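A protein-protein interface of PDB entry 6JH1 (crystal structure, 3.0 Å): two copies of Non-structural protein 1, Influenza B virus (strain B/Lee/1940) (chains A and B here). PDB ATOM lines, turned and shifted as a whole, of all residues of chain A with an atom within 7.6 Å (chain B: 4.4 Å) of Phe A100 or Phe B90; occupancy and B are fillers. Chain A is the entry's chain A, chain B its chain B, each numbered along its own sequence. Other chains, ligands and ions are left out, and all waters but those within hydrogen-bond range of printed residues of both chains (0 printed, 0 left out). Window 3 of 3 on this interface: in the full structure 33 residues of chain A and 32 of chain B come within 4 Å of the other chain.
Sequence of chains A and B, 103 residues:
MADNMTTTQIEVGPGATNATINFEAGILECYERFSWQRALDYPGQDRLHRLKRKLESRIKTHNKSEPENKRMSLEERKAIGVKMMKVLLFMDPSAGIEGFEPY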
ATOM      1  N   ARG A  33     -23.874   6.610  -4.908  1.00  0.00           N
ATOM      2  CA  ARG A  33     -23.697   6.071  -6.224  1.00  0.00           C
ATOM      3  C   ARG A  33     -22.610   5.084  -6.259  1.00  0.00           C
ATOM      4  O   ARG A  33     -22.656   4.122  -6.922  1.00  0.00           O
ATOM      5  CB  ARG A  33     -23.387   7.168  -7.201  1.00  0.00           C
ATOM      6  CG  ARG A  33     -24.231   8.399  -7.074  1.00  0.00           C
ATOM      7  CD  ARG A  33     -24.423   9.090  -8.397  1.00  0.00           C
ATOM      8  NE  ARG A  33     -25.425  10.122  -8.259  1.00  0.00           N
ATOM      9  CZ  ARG A  33     -25.563  11.146  -9.059  1.00  0.00           C
ATOM     10  NH1 ARG A  33     -24.778  11.281 -10.054  1.00  0.00           N
ATOM     11  NH2 ARG A  33     -26.478  12.031  -8.863  1.00  0.00           N
ATOM     12  N   VAL A  82     -23.437  18.022  -6.169  1.00  0.00           N
ATOM     13  CA  VAL A  82     -22.874  17.442  -7.388  1.00  0.00           C
ATOM     14  C   VAL A  82     -22.422  18.548  -8.345  1.00  0.00           C
ATOM     15  O   VAL A  82     -21.391  18.417  -9.001  1.00  0.00           O
ATOM     16  CB  VAL A  82     -23.840  16.422  -8.064  1.00  0.00           C
ATOM     17  CG1 VAL A  82     -24.244  15.353  -7.107  1.00  0.00           C
ATOM     18  CG2 VAL A  82     -25.080  17.074  -8.620  1.00  0.00           C
ATOM     19  N   MET A  85     -19.079  19.794  -7.309  1.00  0.00           N
ATOM     20  CA  MET A  85     -18.100  18.738  -7.514  1.00  0.00           C
ATOM     21  C   MET A  85     -17.680  18.666  -8.970  1.00  0.00           C
ATOM     22  O   MET A  85     -16.491  18.556  -9.269  1.00  0.00           O
ATOM     23  CB  MET A  85     -18.688  17.412  -7.085  1.00  0.00           C
ATOM     24  CG  MET A  85     -19.067  17.378  -5.651  1.00  0.00           C
ATOM     25  SD  MET A  85     -17.812  16.478  -4.842  1.00  0.00           S
ATOM     26  CE  MET A  85     -18.284  14.934  -5.573  1.00  0.00           C
ATOM     27  N   LYS A  86     -18.638  18.713  -9.899  1.00  0.00           N
ATOM     28  CA  LYS A  86     -18.257  18.635 -11.307  1.00  0.00           C
ATOM     29  C   LYS A  86     -17.433  19.845 -11.723  1.00  0.00           C
ATOM     30  O   LYS A  86     -16.590  19.723 -12.621  1.00  0.00           O
ATOM     31  CB  LYS A  86     -19.488  18.477 -12.209  1.00  0.00           C
ATOM     32  CG  LYS A  86     -20.578  17.646 -11.590  1.00  0.00           C
ATOM     33  CD  LYS A  86     -21.917  17.685 -12.270  1.00  0.00           C
ATOM     34  CE  LYS A  86     -22.274  16.417 -12.975  1.00  0.00           C
ATOM     35  NZ  LYS A  86     -23.761  16.490 -13.196  1.00  0.00           N
ATOM     36  N   VAL A  87     -17.653  21.013 -11.086  1.00  0.00           N
ATOM     37  CA  VAL A  87     -16.809  22.161 -11.424  1.00  0.00           C
ATOM     38  C   VAL A  87     -15.406  22.024 -10.806  1.00  0.00           C
ATOM     39  O   VAL A  87     -14.430  22.513 -11.378  1.00  0.00           O
ATOM     40  CB  VAL A  87     -17.457  23.498 -11.008  1.00  0.00           C
ATOM     41  CG1 VAL A  87     -18.902  23.540 -11.411  1.00  0.00           C
ATOM     42  CG2 VAL A  87     -17.242  23.825  -9.563  1.00  0.00           C
ATOM     43  N   LEU A  89     -13.839  19.039 -10.200  1.00  0.00           N
ATOM     44  CA  LEU A  89     -13.182  17.928 -10.867  1.00  0.00           C
ATOM     45  C   LEU A  89     -12.769  18.269 -12.284  1.00  0.00           C
ATOM     46  O   LEU A  89     -11.725  17.807 -12.746  1.00  0.00           O
ATOM     47  CB  LEU A  89     -14.070  16.688 -10.823  1.00  0.00           C
ATOM     48  CG  LEU A  89     -13.582  15.847  -9.647  1.00  0.00           C
ATOM     49  CD1 LEU A  89     -13.407  16.654  -8.425  1.00  0.00           C
ATOM     50  CD2 LEU A  89     -14.463  14.687  -9.340  1.00  0.00           C
ATOM     51  N   PHE A  90     -13.582  19.018 -13.014  1.00  0.00           N
ATOM     52  CA  PHE A  90     -13.159  19.392 -14.351  1.00  0.00           C
ATOM     53  C   PHE A  90     -12.462  20.757 -14.363  1.00  0.00           C
ATOM     54  O   PHE A  90     -12.024  21.214 -15.427  1.00  0.00           O
ATOM     55  CB  PHE A  90     -14.362  19.372 -15.289  1.00  0.00           C
ATOM     56  CG  PHE A  90     -14.832  17.973 -15.629  1.00  0.00           C
ATOM     57  CD1 PHE A  90     -14.211  17.226 -16.634  1.00  0.00           C
ATOM     58  CD2 PHE A  90     -15.924  17.413 -14.957  1.00  0.00           C
ATOM     59  CE1 PHE A  90     -14.650  15.944 -16.943  1.00  0.00           C
ATOM     60  CE2 PHE A  90     -16.368  16.133 -15.264  1.00  0.00           C
ATOM     61  CZ  PHE A  90     -15.735  15.401 -16.260  1.00  0.00           C
ATOM     62  N   SER A  94     -17.690  25.803 -16.453  1.00  0.00           N
ATOM     63  CA  SER A  94     -18.468  25.340 -17.589  1.00  0.00           C
ATOM     64  C   SER A  94     -18.891  23.883 -17.468  1.00  0.00           C
ATOM     65  O   SER A  94     -19.424  23.341 -18.439  1.00  0.00           O
ATOM     66  CB  SER A  94     -17.652  25.532 -18.877  1.00  0.00           C
ATOM     67  OG  SER A  94     -18.167  24.755 -19.945  1.00  0.00           O
ATOM     68  N   ALA A  95     -18.676  23.246 -16.312  1.00  0.00           N
ATOM     69  CA  ALA A  95     -19.099  21.871 -16.067  1.00  0.00           C
ATOM     70  C   ALA A  95     -20.220  21.753 -15.040  1.00  0.00           C
ATOM     71  O   ALA A  95     -20.676  20.632 -14.780  1.00  0.00           O
ATOM     72  CB  ALA A  95     -17.904  21.021 -15.625  1.00  0.00           C
ATOM     73  N   GLY A  96     -20.667  22.876 -14.448  1.00  0.00           N
ATOM     74  CA  GLY A  96     -21.762  22.836 -13.484  1.00  0.00           C
ATOM     75  C   GLY A  96     -23.033  22.195 -14.018  1.00  0.00           C
ATOM     76  O   GLY A  96     -23.675  21.406 -13.320  1.00  0.00           O
ATOM     77  N   ILE A  97     -23.426  22.529 -15.253  1.00  0.00           N
ATOM     78  CA  ILE A  97     -24.517  21.820 -15.929  1.00  0.00           C
ATOM     79  C   ILE A  97     -24.473  22.074 -17.438  1.00  0.00           C
ATOM     80  O   ILE A  97     -25.435  21.768 -18.158  1.00  0.00           O
ATOM     81  CB  ILE A  97     -25.895  22.190 -15.329  1.00  0.00           C
ATOM     82  CG1 ILE A  97     -26.908  21.042 -15.524  1.00  0.00           C
ATOM     83  CG2 ILE A  97     -26.411  23.540 -15.881  1.00  0.00           C
ATOM     84  CD1 ILE A  97     -26.495  19.700 -14.910  1.00  0.00           C
ATOM     85  N   GLU A  98     -23.336  22.601 -17.929  1.00  0.00           N
ATOM     86  CA  GLU A  98     -23.086  22.774 -19.360  1.00  0.00           C
ATOM     87  C   GLU A  98     -21.949  21.897 -19.892  1.00  0.00           C
ATOM     88  O   GLU A  98     -21.918  21.616 -21.096  1.00  0.00           O
ATOM     89  CB  GLU A  98     -22.794  24.260 -19.673  1.00  0.00           C
ATOM     90  CG  GLU A  98     -22.326  24.590 -21.115  1.00  0.00           C
ATOM     91  CD  GLU A  98     -22.885  25.922 -21.678  1.00  0.00           C
ATOM     92  OE1 GLU A  98     -23.885  26.455 -21.136  1.00  0.00           O
ATOM     93  OE2 GLU A  98     -22.326  26.426 -22.686  1.00  0.00           O
ATOM     94  N   GLY A  99     -21.051  21.426 -19.031  1.00  0.00           N
ATOM     95  CA  GLY A  99     -19.927  20.589 -19.445  1.00  0.00           C
ATOM     96  C   GLY A  99     -20.191  19.115 -19.190  1.00  0.00           C
ATOM     97  O   GLY A  99     -20.720  18.737 -18.142  1.00  0.00           O
ATOM     98  N   PHE A 100     -19.815  18.290 -20.163  1.00  0.00           N
ATOM     99  CA  PHE A 100     -20.165  16.881 -20.132  1.00  0.00           C
ATOM    100  C   PHE A 100     -19.007  16.007 -20.594  1.00  0.00           C
ATOM    101  O   PHE A 100     -18.382  16.290 -21.610  1.00  0.00           O
ATOM    102  CB  PHE A 100     -21.409  16.643 -20.996  1.00  0.00           C
ATOM    103  CG  PHE A 100     -22.660  17.289 -20.449  1.00  0.00           C
ATOM    104  CD1 PHE A 100     -22.986  18.601 -20.769  1.00  0.00           C
ATOM    105  CD2 PHE A 100     -23.505  16.583 -19.610  1.00  0.00           C
ATOM    106  CE1 PHE A 100     -24.135  19.198 -20.258  1.00  0.00           C
ATOM    107  CE2 PHE A 100     -24.651  17.169 -19.098  1.00  0.00           C
ATOM    108  CZ  PHE A 100     -24.969  18.478 -19.422  1.00  0.00           C
ATOM    109  N   LYS B  86     -15.553  11.127 -11.589  1.00  0.00           N
ATOM    110  CA  LYS B  86     -16.229  11.672 -12.756  1.00  0.00           C
ATOM    111  C   LYS B  86     -17.215  10.678 -13.367  1.00  0.00           C
ATOM    112  O   LYS B  86     -18.268  11.095 -13.851  1.00  0.00           O
ATOM    113  CB  LYS B  86     -15.221  12.145 -13.795  1.00  0.00           C
ATOM    114  CG  LYS B  86     -13.996  12.677 -13.195  1.00  0.00           C
ATOM    115  CD  LYS B  86     -12.922  12.973 -14.204  1.00  0.00           C
ATOM    116  CE  LYS B  86     -12.800  14.478 -14.353  1.00  0.00           C
ATOM    117  NZ  LYS B  86     -11.504  14.859 -14.962  1.00  0.00           N
ATOM    118  N   VAL B  87     -16.949   9.373 -13.299  1.00  0.00           N
ATOM    119  CA  VAL B  87     -17.943   8.471 -13.859  1.00  0.00           C
ATOM    120  C   VAL B  87     -19.163   8.422 -12.947  1.00  0.00           C
ATOM    121  O   VAL B  87     -20.285   8.250 -13.424  1.00  0.00           O
ATOM    122  CB  VAL B  87     -17.371   7.060 -14.080  1.00  0.00           C
ATOM    123  CG1 VAL B  87     -16.020   7.145 -14.722  1.00  0.00           C
ATOM    124  CG2 VAL B  87     -17.402   6.226 -12.832  1.00  0.00           C
ATOM    125  N   LEU B  88     -18.979   8.598 -11.631  1.00  0.00           N
ATOM    126  CA  LEU B  88     -20.132   8.585 -10.741  1.00  0.00           C
ATOM    127  C   LEU B  88     -21.000   9.827 -10.922  1.00  0.00           C
ATOM    128  O   LEU B  88     -22.229   9.731 -10.921  1.00  0.00           O
ATOM    129  CB  LEU B  88     -19.683   8.446  -9.296  1.00  0.00           C
ATOM    130  CG  LEU B  88     -19.127   7.047  -9.029  1.00  0.00           C
ATOM    131  CD1 LEU B  88     -18.891   6.920  -7.553  1.00  0.00           C
ATOM    132  CD2 LEU B  88     -19.949   5.888  -9.559  1.00  0.00           C
ATOM    133  N   LEU B  89     -20.390  10.999 -11.070  1.00  0.00           N
ATOM    134  CA  LEU B  89     -21.164  12.236 -11.189  1.00  0.00           C
ATOM    135  C   LEU B  89     -21.929  12.312 -12.500  1.00  0.00           C
ATOM    136  O   LEU B  89     -23.078  12.766 -12.531  1.00  0.00           O
ATOM    137  CB  LEU B  89     -20.233  13.442 -11.087  1.00  0.00           C
ATOM    138  CG  LEU B  89     -19.880  14.129  -9.787  1.00  0.00           C
ATOM    139  CD1 LEU B  89     -19.533  13.122  -8.824  1.00  0.00           C
ATOM    140  CD2 LEU B  89     -18.620  14.903 -10.099  1.00  0.00           C
ATOM    141  N   PHE B  90     -21.301  11.914 -13.592  1.00  0.00           N
ATOM    142  CA  PHE B  90     -21.962  11.932 -14.874  1.00  0.00           C
ATOM    143  C   PHE B  90     -22.599  10.601 -15.225  1.00  0.00           C
ATOM    144  O   PHE B  90     -23.132  10.460 -16.334  1.00  0.00           O
ATOM    145  CB  PHE B  90     -20.981  12.371 -15.946  1.00  0.00           C
ATOM    146  CG  PHE B  90     -20.720  13.830 -15.915  1.00  0.00           C
ATOM    147  CD1 PHE B  90     -21.610  14.704 -16.529  1.00  0.00           C
ATOM    148  CD2 PHE B  90     -19.646  14.347 -15.215  1.00  0.00           C
ATOM    149  CE1 PHE B  90     -21.409  16.065 -16.487  1.00  0.00           C
ATOM    150  CE2 PHE B  90     -19.438  15.704 -15.158  1.00  0.00           C
ATOM    151  CZ  PHE B  90     -20.314  16.569 -15.796  1.00  0.00           C
ATOM    152  N   MET B  91     -22.568   9.630 -14.303  1.00  0.00           N
ATOM    153  CA  MET B  91     -23.080   8.285 -14.534  1.00  0.00           C
ATOM    154  C   MET B  91     -22.718   7.733 -15.907  1.00  0.00           C
ATOM    155  O   MET B  91     -23.453   6.914 -16.458  1.00  0.00           O
ATOM    156  CB  MET B  91     -24.587   8.288 -14.313  1.00  0.00           C
ATOM    157  CG  MET B  91     -24.951   8.175 -12.839  1.00  0.00           C
ATOM    158  SD  MET B  91     -24.206   6.685 -12.145  1.00  0.00           S
ATOM    159  CE  MET B  91     -24.703   6.808 -10.462  1.00  0.00           C
ATOM    160  N   ASP B  92     -21.582   8.165 -16.447  1.00  0.00           N
ATOM    161  CA  ASP B  92     -21.051   7.758 -17.728  1.00  0.00           C
ATOM    162  C   ASP B  92     -19.695   7.116 -17.491  1.00  0.00           C
ATOM    163  O   ASP B  92     -18.861   7.700 -16.789  1.00  0.00           O
ATOM    164  CB  ASP B  92     -20.869   8.961 -18.685  1.00  0.00           C
ATOM    165  CG  ASP B  92     -21.978   9.097 -19.698  1.00  0.00           C
ATOM    166  OD1 ASP B  92     -22.185   8.142 -20.481  1.00  0.00           O
ATOM    167  OD2 ASP B  92     -22.609  10.177 -19.746  1.00  0.00           O
ATOM    168  N   GLY B  99     -13.085  13.166 -21.452  1.00  0.00           N
ATOM    169  CA  GLY B  99     -14.445  13.536 -21.825  1.00  0.00           C
ATOM    170  C   GLY B  99     -15.007  14.685 -21.015  1.00  0.00           C
ATOM    171  O   GLY B  99     -16.165  15.044 -21.174  1.00  0.00           O
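Phe A100 touches just these residues of chain B: Phe B90 (3.8 Å) and Gly B99 (2.6 Å). Of chain A, only Lys A86 (3.4 Å), Phe A90 (3.1 Å), Gly A99 (3.2 Å) and Phe A100 (3.8 Å) come within 4 Å of Phe B90. Of the printed residues of chain B, Leu A89 touches Lys B86. Printed residues of chain A within 4 Å of Met B91: Arg A33 (3.1 Å). The nearest printed residue of chain B that does not touch Leu A89 is Leu B89 (4.2 Å).
Of the 14 printed residues of chain A, 7 touch a printed residue of chain B. Printed residues of chain A that touch a printed residue of chain B: Arg A33, Met A85, Lys A86, Leu A89, Phe A90, Gly A99 and Phe A100. Hydrophobic or aromatic side chains of chain A within 4 Å of the printed part of chain B: Met A85, Phe A90 and Phe A100. Printed residues of chain B that touch a printed residue of chain A: Lys B86, Leu B88, Leu B89, Phe B90, Met B91 and Gly B99. Hydrophobic or aromatic side chains of chain B that line the printed part of chain A: Leu B89, Phe B90 and Met B91. Among the printed residues, 12 pairs touch across the chains.
O of Leu B88 lies within hydrogen-bond range of NH1 of Arg A33 (3.1 Å). The guanidinium group (NH1) of Arg A33 sits at hydrogen-bond distance from the backbone carbonyl oxygen (O) of Leu B89 (3.4 Å). The backbone carbonyl oxygen (O) of Phe A100 sits close to the backbone carbonyl oxygen (O) of Gly B99 (2.6 Å).
The backbone carbonyl oxygen (O) of Ser A94 is in hydrogen-bond range of the backbone NH (N) of Gly A99 (2.6 Å).
Among the printed residues, merely in contact across the chains: Arg A33 with Met B91, Met A85 with Leu B89, Lys A86 with Leu B89, Lys A86 with Phe B90, Leu A89 with Lys B86, Phe A90 with Lys B86, Phe A90 with Phe B90, Gly A99 with Phe B90 and Phe A100 with Phe B90.
Lys A86 touches Leu B89, and with the chains exchanged Leu A89 touches Lys B86. Lys A86 touches Phe B90, and with the chains exchanged Phe A90 touches Lys B86. Phe A90 touches its own counterpart, Phe B90. Gly A99 touches Phe B90, but with the chains exchanged Phe A90 does not touch Gly B99 (4.3 Å). Positions printed for both chains: 86, 87, 89, 90 and 99.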
